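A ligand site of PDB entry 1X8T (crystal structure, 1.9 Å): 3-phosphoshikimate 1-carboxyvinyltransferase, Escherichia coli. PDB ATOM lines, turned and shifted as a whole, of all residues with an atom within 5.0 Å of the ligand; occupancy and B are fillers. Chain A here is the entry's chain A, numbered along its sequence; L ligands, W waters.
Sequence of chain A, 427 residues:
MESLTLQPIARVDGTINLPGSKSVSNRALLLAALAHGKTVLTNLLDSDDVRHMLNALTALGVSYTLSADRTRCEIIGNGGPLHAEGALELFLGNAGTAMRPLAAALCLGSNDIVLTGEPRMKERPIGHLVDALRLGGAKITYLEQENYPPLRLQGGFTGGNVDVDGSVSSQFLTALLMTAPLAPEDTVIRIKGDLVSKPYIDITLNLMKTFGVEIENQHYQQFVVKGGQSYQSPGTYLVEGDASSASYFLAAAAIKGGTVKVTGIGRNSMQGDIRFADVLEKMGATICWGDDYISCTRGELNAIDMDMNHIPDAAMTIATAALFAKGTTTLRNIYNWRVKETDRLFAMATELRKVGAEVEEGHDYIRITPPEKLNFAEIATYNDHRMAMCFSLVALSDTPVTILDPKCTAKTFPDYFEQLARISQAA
The side-chain hydroxyl (OG) of Ser 169 is in hydrogen-bond range of the backbone NH (N) of Gln 171, at 3.1 Å. A ring nitrogen (NE2) of His 385 sits at hydrogen-bond distance from the guanidinium group of Arg 344 (3.5 Å). A ring nitrogen (ND1) of His 385 lies within hydrogen-bond range of the side-chain hydroxyl (OG1) of Thr 412, at 2.9 Å. The guanidinium group (NH2) of Arg 27 lies within hydrogen-bond range of the backbone carbonyl oxygen (O) of Ser 23, at 3.1 Å. The guanidinium group (NH1) of Arg 27 lies within hydrogen-bond range of the backbone carbonyl oxygen (O) of Tyr 200 (3.2 Å). NH2 of Arg 344 lies within salt-bridge range of OD2 of Asp 313 (3.4 Å). The side-chain carboxylate (OE2) of Glu 341 is in salt-bridge range of the side-chain amino group (NZ) of Lys 411 (3.7 Å). The side-chain amino group (NZ) of Lys 411 lies within salt-bridge range of the side-chain carboxylate (OD1) of Asp 49, 2.7 Å away.
The side-chain hydroxyl of Ser 197 is in hydrogen-bond range of an oxygen (O7) of the ligand (2.5 Å). The side-chain hydroxyl (OG) of Ser 169 sits at hydrogen-bond distance from an oxygen (O8) of the ligand. N of Ser 170 sits at hydrogen-bond distance from O6 of the ligand (2.8 Å). O6 of the ligand lies within hydrogen-bond range of OG of Ser 170 (2.6 Å). O7 of the ligand is in salt-bridge range of NZ of Lys 340. NZ of Lys 22 lies within salt-bridge range of O9 of the ligand (2.6 Å). An oxygen (O13) of the ligand lies within hydrogen-bond range of a ring nitrogen (NE2) of His 385, 2.7 Å away. The guanidinium group (NH1) of Arg 27 is in salt-bridge range of an oxygen (O4) of the ligand. OD2 of Asp 313 sits at hydrogen-bond distance from O2 of the ligand (2.9 Å). An oxygen (O7) of the ligand lies close to the side-chain amide oxygen (OD1) of Asn 336, at 2.8 Å. The side-chain hydroxyl (OG) of Ser 23 lies within hydrogen-bond range of an oxygen (O5) of the ligand (2.8 Å). The guanidinium group (NE) of Arg 386 is in salt-bridge range of an oxygen (O11) of the ligand, 2.9 Å away. NE2 of Gln 171 lies within hydrogen-bond range of O1 of the ligand, at 3.0 Å. O11 of the ligand lies within salt-bridge range of NH2 of Arg 344 (3.0 Å).
Water W1 lies within hydrogen-bond range of O8 of the ligand, O of Val 168 and OD1 of Asn 336. Water W6 lies within hydrogen-bond range of O4 of the ligand (2.7 Å), OG1 of Thr 174 (2.7 Å), OG of Ser 170 (2.8 Å), NH1 of Arg 27 (3.3 Å) and N of Gln 171 (3.3 Å). Water W2 lies within hydrogen-bond range of NZ of Lys 411 (2.7 Å), N of Gly 96 (2.9 Å), O10 of the ligand (2.9 Å) and OE2 of Glu 341 (3.4 Å). Water W8 lies within hydrogen-bond range of the side-chain amide nitrogen of Gln 171 (2.7 Å), an oxygen (O8) of the ligand (2.9 Å) and the guanidinium group of Arg 100 (3.2 Å). Water W3 bridges OE1 of Gln 171 (2.7 Å) and O9 of the ligand (3.1 Å). Water W4 lies within hydrogen-bond range of the side-chain carboxylate of Glu 341 (2.7 Å) and an oxygen (O10) of the ligand (3.2 Å).
Merely in contact with the ligand: Tyr 200, Glu 341, Thr 97 and Lys 411. Hydrophobic or aromatic side chains within 4 Å of the ligand: Tyr 200 and His 385.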
ATOM      1  N   LYS A  22      28.025  13.473   1.633  1.00  0.00           N
ATOM      2  CA  LYS A  22      26.940  14.273   2.193  1.00  0.00           C
ATOM      3  C   LYS A  22      26.832  14.002   3.694  1.00  0.00           C
ATOM      4  O   LYS A  22      26.641  14.915   4.488  1.00  0.00           O
ATOM      5  CB  LYS A  22      25.606  13.933   1.502  1.00  0.00           C
ATOM      6  CG  LYS A  22      24.398  14.599   2.144  1.00  0.00           C
ATOM      7  CD  LYS A  22      23.569  13.595   2.944  1.00  0.00           C
ATOM      8  CE  LYS A  22      22.810  12.650   2.014  1.00  0.00           C
ATOM      9  NZ  LYS A  22      22.207  11.499   2.751  1.00  0.00           N
ATOM     10  N   SER A  23      26.964  12.729   4.070  1.00  0.00           N
ATOM     11  CA  SER A  23      26.877  12.326   5.470  1.00  0.00           C
ATOM     12  C   SER A  23      27.938  13.019   6.307  1.00  0.00           C
ATOM     13  O   SER A  23      27.652  13.568   7.361  1.00  0.00           O
ATOM     14  CB  SER A  23      27.021  10.810   5.585  1.00  0.00           C
ATOM     15  OG  SER A  23      25.868  10.168   5.091  1.00  0.00           O
ATOM     16  N   ARG A  27      27.445  16.519   8.990  1.00  0.00           N
ATOM     17  CA  ARG A  27      27.844  16.295  10.369  1.00  0.00           C
ATOM     18  C   ARG A  27      28.946  17.310  10.694  1.00  0.00           C
ATOM     19  O   ARG A  27      28.950  17.946  11.753  1.00  0.00           O
ATOM     20  CB  ARG A  27      28.399  14.895  10.548  1.00  0.00           C
ATOM     21  CG  ARG A  27      27.359  13.778  10.572  1.00  0.00           C
ATOM     22  CD  ARG A  27      28.069  12.453  10.526  1.00  0.00           C
ATOM     23  NE  ARG A  27      27.209  11.304  10.811  1.00  0.00           N
ATOM     24  CZ  ARG A  27      26.237  10.871  10.019  1.00  0.00           C
ATOM     25  NH1 ARG A  27      25.527   9.806  10.386  1.00  0.00           N
ATOM     26  NH2 ARG A  27      25.956  11.494   8.873  1.00  0.00           N
ATOM     27  N   ASP A  49      21.397  19.084  -0.214  1.00  0.00           N
ATOM     28  CA  ASP A  49      21.412  18.720   1.201  1.00  0.00           C
ATOM     29  C   ASP A  49      22.366  19.600   1.998  1.00  0.00           C
ATOM     30  O   ASP A  49      22.049  20.037   3.103  1.00  0.00           O
ATOM     31  CB  ASP A  49      21.792  17.237   1.382  1.00  0.00           C
ATOM     32  CG  ASP A  49      20.568  16.314   1.436  1.00  0.00           C
ATOM     33  OD1 ASP A  49      19.426  16.800   1.278  1.00  0.00           O
ATOM     34  OD2 ASP A  49      20.759  15.092   1.645  1.00  0.00           O
ATOM     35  N   GLY A  96      17.401  15.808   5.410  1.00  0.00           N
ATOM     36  CA  GLY A  96      17.105  15.038   6.606  1.00  0.00           C
ATOM     37  C   GLY A  96      18.303  15.015   7.537  1.00  0.00           C
ATOM     38  O   GLY A  96      18.151  14.912   8.753  1.00  0.00           O
ATOM     39  N   THR A  97      19.493  15.088   6.960  1.00  0.00           N
ATOM     40  CA  THR A  97      20.683  15.096   7.792  1.00  0.00           C
ATOM     41  C   THR A  97      20.869  16.468   8.447  1.00  0.00           C
ATOM     42  O   THR A  97      21.871  16.719   9.127  1.00  0.00           O
ATOM     43  CB  THR A  97      21.940  14.711   6.980  1.00  0.00           C
ATOM     44  OG1 THR A  97      21.962  15.446   5.756  1.00  0.00           O
ATOM     45  CG2 THR A  97      21.944  13.201   6.708  1.00  0.00           C
ATOM     46  N   ARG A 100      17.117  15.990  11.341  1.00  0.00           N
ATOM     47  CA  ARG A 100      17.327  15.150  12.498  1.00  0.00           C
ATOM     48  C   ARG A 100      18.354  15.702  13.491  1.00  0.00           C
ATOM     49  O   ARG A 100      18.041  15.873  14.668  1.00  0.00           O
ATOM     50  CB  ARG A 100      17.703  13.719  12.068  1.00  0.00           C
ATOM     51  CG  ARG A 100      16.503  12.788  11.753  1.00  0.00           C
ATOM     52  CD  ARG A 100      15.764  13.189  10.470  1.00  0.00           C
ATOM     53  NE  ARG A 100      14.669  12.276  10.133  1.00  0.00           N
ATOM     54  CZ  ARG A 100      14.812  11.095   9.540  1.00  0.00           C
ATOM     55  NH1 ARG A 100      13.742  10.348   9.268  1.00  0.00           N
ATOM     56  NH2 ARG A 100      16.008  10.663   9.194  1.00  0.00           N
ATOM     57  N   VAL A 168      14.254   1.908  13.072  1.00  0.00           N
ATOM     58  CA  VAL A 168      13.806   2.502  11.818  1.00  0.00           C
ATOM     59  C   VAL A 168      14.896   3.373  11.194  1.00  0.00           C
ATOM     60  O   VAL A 168      15.079   3.366   9.972  1.00  0.00           O
ATOM     61  CB  VAL A 168      12.528   3.333  12.000  1.00  0.00           C
ATOM     62  CG1 VAL A 168      12.226   4.120  10.722  1.00  0.00           C
ATOM     63  CG2 VAL A 168      11.358   2.412  12.339  1.00  0.00           C
ATOM     64  N   SER A 169      15.616   4.117  12.024  1.00  0.00           N
ATOM     65  CA  SER A 169      16.684   4.960  11.482  1.00  0.00           C
ATOM     66  C   SER A 169      17.824   5.155  12.466  1.00  0.00           C
ATOM     67  O   SER A 169      17.612   5.403  13.640  1.00  0.00           O
ATOM     68  CB  SER A 169      16.125   6.336  11.100  1.00  0.00           C
ATOM     69  OG  SER A 169      17.145   7.140  10.541  1.00  0.00           O
ATOM     70  N   SER A 170      19.048   5.058  11.951  1.00  0.00           N
ATOM     71  CA  SER A 170      20.235   5.254  12.763  1.00  0.00           C
ATOM     72  C   SER A 170      20.379   6.754  13.001  1.00  0.00           C
ATOM     73  O   SER A 170      21.086   7.188  13.905  1.00  0.00           O
ATOM     74  CB  SER A 170      21.486   4.766  12.034  1.00  0.00           C
ATOM     75  OG  SER A 170      21.790   5.619  10.938  1.00  0.00           O
ATOM     76  N   GLN A 171      19.700   7.563  12.181  1.00  0.00           N
ATOM     77  CA  GLN A 171      19.815   9.011  12.311  1.00  0.00           C
ATOM     78  C   GLN A 171      19.315   9.597  13.622  1.00  0.00           C
ATOM     79  O   GLN A 171      19.794  10.650  14.056  1.00  0.00           O
ATOM     80  CB  GLN A 171      19.109   9.707  11.157  1.00  0.00           C
ATOM     81  CG  GLN A 171      19.748   9.425   9.809  1.00  0.00           C
ATOM     82  CD  GLN A 171      19.037  10.149   8.685  1.00  0.00           C
ATOM     83  OE1 GLN A 171      18.930  11.371   8.707  1.00  0.00           O
ATOM     84  NE2 GLN A 171      18.558   9.396   7.711  1.00  0.00           N
ATOM     85  N   THR A 174      22.124   9.094  15.902  1.00  0.00           N
ATOM     86  CA  THR A 174      23.175  10.025  15.471  1.00  0.00           C
ATOM     87  C   THR A 174      22.923  11.424  16.027  1.00  0.00           C
ATOM     88  O   THR A 174      23.830  12.068  16.571  1.00  0.00           O
ATOM     89  CB  THR A 174      23.258  10.061  13.934  1.00  0.00           C
ATOM     90  OG1 THR A 174      24.110   9.000  13.498  1.00  0.00           O
ATOM     91  CG2 THR A 174      23.804  11.407  13.450  1.00  0.00           C
ATOM     92  N   VAL A 196      19.507  -0.245  13.075  1.00  0.00           N
ATOM     93  CA  VAL A 196      19.717  -0.385  11.645  1.00  0.00           C
ATOM     94  C   VAL A 196      20.730   0.662  11.170  1.00  0.00           C
ATOM     95  O   VAL A 196      21.002   1.642  11.874  1.00  0.00           O
ATOM     96  CB  VAL A 196      18.400  -0.216  10.855  1.00  0.00           C
ATOM     97  CG1 VAL A 196      17.415  -1.302  11.238  1.00  0.00           C
ATOM     98  CG2 VAL A 196      17.810   1.171  11.099  1.00  0.00           C
ATOM     99  N   SER A 197      21.282   0.432   9.987  1.00  0.00           N
ATOM    100  CA  SER A 197      22.246   1.366   9.404  1.00  0.00           C
ATOM    101  C   SER A 197      23.346   1.696  10.395  1.00  0.00           C
ATOM    102  O   SER A 197      23.772   2.839  10.509  1.00  0.00           O
ATOM    103  CB  SER A 197      21.523   2.650   8.981  1.00  0.00           C
ATOM    104  OG  SER A 197      20.577   2.379   7.970  1.00  0.00           O
ATOM    105  N   TYR A 200      26.482   4.136   9.959  1.00  0.00           N
ATOM    106  CA  TYR A 200      26.345   5.588  10.039  1.00  0.00           C
ATOM    107  C   TYR A 200      26.629   6.084  11.455  1.00  0.00           C
ATOM    108  O   TYR A 200      27.023   7.226  11.651  1.00  0.00           O
ATOM    109  CB  TYR A 200      24.956   6.021   9.577  1.00  0.00           C
ATOM    110  CG  TYR A 200      24.783   5.827   8.098  1.00  0.00           C
ATOM    111  CD1 TYR A 200      24.205   4.671   7.580  1.00  0.00           C
ATOM    112  CD2 TYR A 200      25.240   6.800   7.195  1.00  0.00           C
ATOM    113  CE1 TYR A 200      24.079   4.485   6.200  1.00  0.00           C
ATOM    114  CE2 TYR A 200      25.121   6.622   5.824  1.00  0.00           C
ATOM    115  CZ  TYR A 200      24.539   5.464   5.333  1.00  0.00           C
ATOM    116  OH  TYR A 200      24.449   5.290   3.973  1.00  0.00           O
ATOM    117  N   PRO A 312      22.215   0.277   3.241  1.00  0.00           N
ATOM    118  CA  PRO A 312      20.899   0.508   2.649  1.00  0.00           C
ATOM    119  C   PRO A 312      20.842   1.336   1.367  1.00  0.00           C
ATOM    120  O   PRO A 312      20.114   0.993   0.447  1.00  0.00           O
ATOM    121  CB  PRO A 312      20.116   1.167   3.797  1.00  0.00           C
ATOM    122  CG  PRO A 312      21.197   1.892   4.560  1.00  0.00           C
ATOM    123  CD  PRO A 312      22.310   0.877   4.579  1.00  0.00           C
ATOM    124  N   ASP A 313      21.623   2.409   1.302  1.00  0.00           N
ATOM    125  CA  ASP A 313      21.609   3.279   0.129  1.00  0.00           C
ATOM    126  C   ASP A 313      22.349   2.658  -1.042  1.00  0.00           C
ATOM    127  O   ASP A 313      21.809   2.576  -2.148  1.00  0.00           O
ATOM    128  CB  ASP A 313      22.200   4.635   0.486  1.00  0.00           C
ATOM    129  CG  ASP A 313      21.311   5.428   1.418  1.00  0.00           C
ATOM    130  OD1 ASP A 313      21.718   6.530   1.848  1.00  0.00           O
ATOM    131  OD2 ASP A 313      20.183   4.956   1.719  1.00  0.00           O
ATOM    132  N   ASN A 336      13.725   0.053   5.882  1.00  0.00           N
ATOM    133  CA  ASN A 336      13.686   1.508   5.867  1.00  0.00           C
ATOM    134  C   ASN A 336      13.861   2.177   4.506  1.00  0.00           C
ATOM    135  O   ASN A 336      13.914   3.398   4.397  1.00  0.00           O
ATOM    136  CB  ASN A 336      14.584   2.128   6.979  1.00  0.00           C
ATOM    137  CG  ASN A 336      16.055   2.194   6.634  1.00  0.00           C
ATOM    138  OD1 ASN A 336      16.873   2.543   7.508  1.00  0.00           O
ATOM    139  ND2 ASN A 336      16.412   1.898   5.402  1.00  0.00           N
ATOM    140  N   LYS A 340      12.240   6.594   3.282  1.00  0.00           N
ATOM    141  CA  LYS A 340      13.182   7.612   2.853  1.00  0.00           C
ATOM    142  C   LYS A 340      12.635   8.563   1.795  1.00  0.00           C
ATOM    143  O   LYS A 340      11.432   8.831   1.805  1.00  0.00           O
ATOM    144  CB  LYS A 340      14.482   6.927   2.435  1.00  0.00           C
ATOM    145  CG  LYS A 340      15.233   6.479   3.679  1.00  0.00           C
ATOM    146  CD  LYS A 340      16.347   5.474   3.442  1.00  0.00           C
ATOM    147  CE  LYS A 340      17.061   5.236   4.770  1.00  0.00           C
ATOM    148  NZ  LYS A 340      18.262   4.337   4.623  1.00  0.00           N
ATOM    149  N   GLU A 341      13.480   9.100   0.909  1.00  0.00           N
ATOM    150  CA  GLU A 341      13.016  10.065  -0.096  1.00  0.00           C
ATOM    151  C   GLU A 341      11.699   9.670  -0.760  1.00  0.00           C
ATOM    152  O   GLU A 341      10.922  10.525  -1.181  1.00  0.00           O
ATOM    153  CB  GLU A 341      14.093  10.288  -1.166  1.00  0.00           C
ATOM    154  CG  GLU A 341      15.267  11.087  -0.628  1.00  0.00           C
ATOM    155  CD  GLU A 341      14.838  12.441  -0.076  1.00  0.00           C
ATOM    156  OE1 GLU A 341      14.638  13.371  -0.874  1.00  0.00           O
ATOM    157  OE2 GLU A 341      14.692  12.544   1.165  1.00  0.00           O
ATOM    158  N   ARG A 344      11.327   3.395  -1.391  1.00  0.00           N
ATOM    159  CA  ARG A 344      12.240   2.809  -2.360  1.00  0.00           C
ATOM    160  C   ARG A 344      11.975   1.358  -2.709  1.00  0.00           C
ATOM    161  O   ARG A 344      12.368   0.903  -3.778  1.00  0.00           O
ATOM    162  CB  ARG A 344      13.676   3.014  -1.869  1.00  0.00           C
ATOM    163  CG  ARG A 344      14.046   4.489  -1.920  1.00  0.00           C
ATOM    164  CD  ARG A 344      15.355   4.773  -1.209  1.00  0.00           C
ATOM    165  NE  ARG A 344      15.820   6.120  -1.510  1.00  0.00           N
ATOM    166  CZ  ARG A 344      16.826   6.723  -0.872  1.00  0.00           C
ATOM    167  NH1 ARG A 344      17.177   7.960  -1.216  1.00  0.00           N
ATOM    168  NH2 ARG A 344      17.463   6.105   0.117  1.00  0.00           N
ATOM    169  N   HIS A 385      16.767  11.300  -5.500  1.00  0.00           N
ATOM    170  CA  HIS A 385      18.059  11.341  -6.181  1.00  0.00           C
ATOM    171  C   HIS A 385      18.626   9.964  -6.512  1.00  0.00           C
ATOM    172  O   HIS A 385      19.214   9.766  -7.581  1.00  0.00           O
ATOM    173  CB  HIS A 385      19.091  12.113  -5.341  1.00  0.00           C
ATOM    174  CG  HIS A 385      19.266  11.592  -3.956  1.00  0.00           C
ATOM    175  ND1 HIS A 385      20.464  11.668  -3.274  1.00  0.00           N
ATOM    176  CD2 HIS A 385      18.385  11.042  -3.089  1.00  0.00           C
ATOM    177  CE1 HIS A 385      20.311  11.194  -2.052  1.00  0.00           C
ATOM    178  NE2 HIS A 385      19.058  10.802  -1.916  1.00  0.00           N
ATOM    179  N   ARG A 386      18.441   8.990  -5.620  1.00  0.00           N
ATOM    180  CA  ARG A 386      19.009   7.672  -5.890  1.00  0.00           C
ATOM    181  C   ARG A 386      18.260   6.864  -6.942  1.00  0.00           C
ATOM    182  O   ARG A 386      18.853   6.001  -7.593  1.00  0.00           O
ATOM    183  CB  ARG A 386      19.156   6.885  -4.586  1.00  0.00           C
ATOM    184  CG  ARG A 386      20.021   7.633  -3.582  1.00  0.00           C
ATOM    185  CD  ARG A 386      20.568   6.762  -2.439  1.00  0.00           C
ATOM    186  NE  ARG A 386      21.288   7.608  -1.500  1.00  0.00           N
ATOM    187  CZ  ARG A 386      22.465   8.188  -1.745  1.00  0.00           C
ATOM    188  NH1 ARG A 386      23.022   8.958  -0.831  1.00  0.00           N
ATOM    189  NH2 ARG A 386      23.098   7.956  -2.889  1.00  0.00           N
ATOM    190  N   LYS A 411      20.250  16.546  -4.911  1.00  0.00           N
ATOM    191  CA  LYS A 411      20.181  16.391  -3.460  1.00  0.00           C
ATOM    192  C   LYS A 411      21.586  16.059  -2.923  1.00  0.00           C
ATOM    193  O   LYS A 411      22.012  16.624  -1.913  1.00  0.00           O
ATOM    194  CB  LYS A 411      19.189  15.293  -3.072  1.00  0.00           C
ATOM    195  CG  LYS A 411      19.040  15.129  -1.567  1.00  0.00           C
ATOM    196  CD  LYS A 411      18.108  13.973  -1.227  1.00  0.00           C
ATOM    197  CE  LYS A 411      18.146  13.661   0.266  1.00  0.00           C
ATOM    198  NZ  LYS A 411      17.640  14.801   1.085  1.00  0.00           N
ATOM    199  N   THR A 412      22.291  15.172  -3.613  1.00  0.00           N
ATOM    200  CA  THR A 412      23.627  14.781  -3.195  1.00  0.00           C
ATOM    201  C   THR A 412      24.662  14.792  -4.316  1.00  0.00           C
ATOM    202  O   THR A 412      25.864  14.703  -4.048  1.00  0.00           O
ATOM    203  CB  THR A 412      23.666  13.344  -2.643  1.00  0.00           C
ATOM    204  OG1 THR A 412      23.188  12.426  -3.645  1.00  0.00           O
ATOM    205  CG2 THR A 412      22.816  13.224  -1.402  1.00  0.00           C
HETATM  206  C1  LIG L   1      22.380   8.883   6.944  1.00  0.00           C
HETATM  207  C2  LIG L   1      21.983   7.557   7.383  1.00  0.00           C
HETATM  208  C3  LIG L   1      21.082   6.693   6.486  1.00  0.00           C
HETATM  209  C4  LIG L   1      21.086   7.145   4.938  1.00  0.00           C
HETATM  210  C5  LIG L   1      20.716   8.664   4.882  1.00  0.00           C
HETATM  211  C6  LIG L   1      21.910   9.449   5.607  1.00  0.00           C
HETATM  212  C7  LIG L   1      23.262   9.734   7.787  1.00  0.00           C
HETATM  213  O1  LIG L   1      19.608   6.707   7.080  1.00  0.00           O
HETATM  214  O2  LIG L   1      20.153   6.259   4.307  1.00  0.00           O
HETATM  215  O3  LIG L   1      20.656   9.114   3.555  1.00  0.00           O
HETATM  216  O4  LIG L   1      23.169   9.646   9.005  1.00  0.00           O
HETATM  217  O5  LIG L   1      24.030  10.450   7.185  1.00  0.00           O
HETATM  218  P1  LIG L   1      18.952   5.498   8.033  1.00  0.00           P
HETATM  219  O6  LIG L   1      19.819   5.449   9.302  1.00  0.00           O
HETATM  220  O7  LIG L   1      19.071   4.221   7.122  1.00  0.00           O
HETATM  221  O8  LIG L   1      17.547   6.104   8.261  1.00  0.00           O
HETATM  222  C8  LIG L   1      19.311   9.444   3.060  1.00  0.00           C
HETATM  223  C9  LIG L   1      17.982   8.555   3.368  1.00  0.00           C
HETATM  224  C10 LIG L   1      19.328  10.947   3.570  1.00  0.00           C
HETATM  225  O9  LIG L   1      20.003  11.841   4.171  1.00  0.00           O
HETATM  226  O10 LIG L   1      18.162  11.146   3.143  1.00  0.00           O
HETATM  227  P2  LIG L   1      19.564   9.517   1.224  1.00  0.00           P
HETATM  228  O11 LIG L   1      19.632   8.019   0.861  1.00  0.00           O
HETATM  229  O12 LIG L   1      20.822  10.239   0.801  1.00  0.00           O
HETATM  230  O13 LIG L   1      18.278  10.109   0.608  1.00  0.00           O
HETATM  231  O   HOH W   1      15.025   5.249   8.019  1.00  0.00           O
HETATM  232  O   HOH W   2      16.927  13.760   3.460  1.00  0.00           O
HETATM  233  O   HOH W   3      17.810  11.706   6.297  1.00  0.00           O
HETATM  234  O   HOH W   4      15.114  10.376   2.739  1.00  0.00           O
HETATM  235  O   HOH W   5      22.655  12.250  10.092  1.00  0.00           O
HETATM  236  O   HOH W   6      22.825   8.169  11.238  1.00  0.00           O
HETATM  237  O   HOH W   7      20.061  14.349   4.110  1.00  0.00           O
HETATM  238  O   HOH W   8      16.200   8.401   6.998  1.00  0.00           O
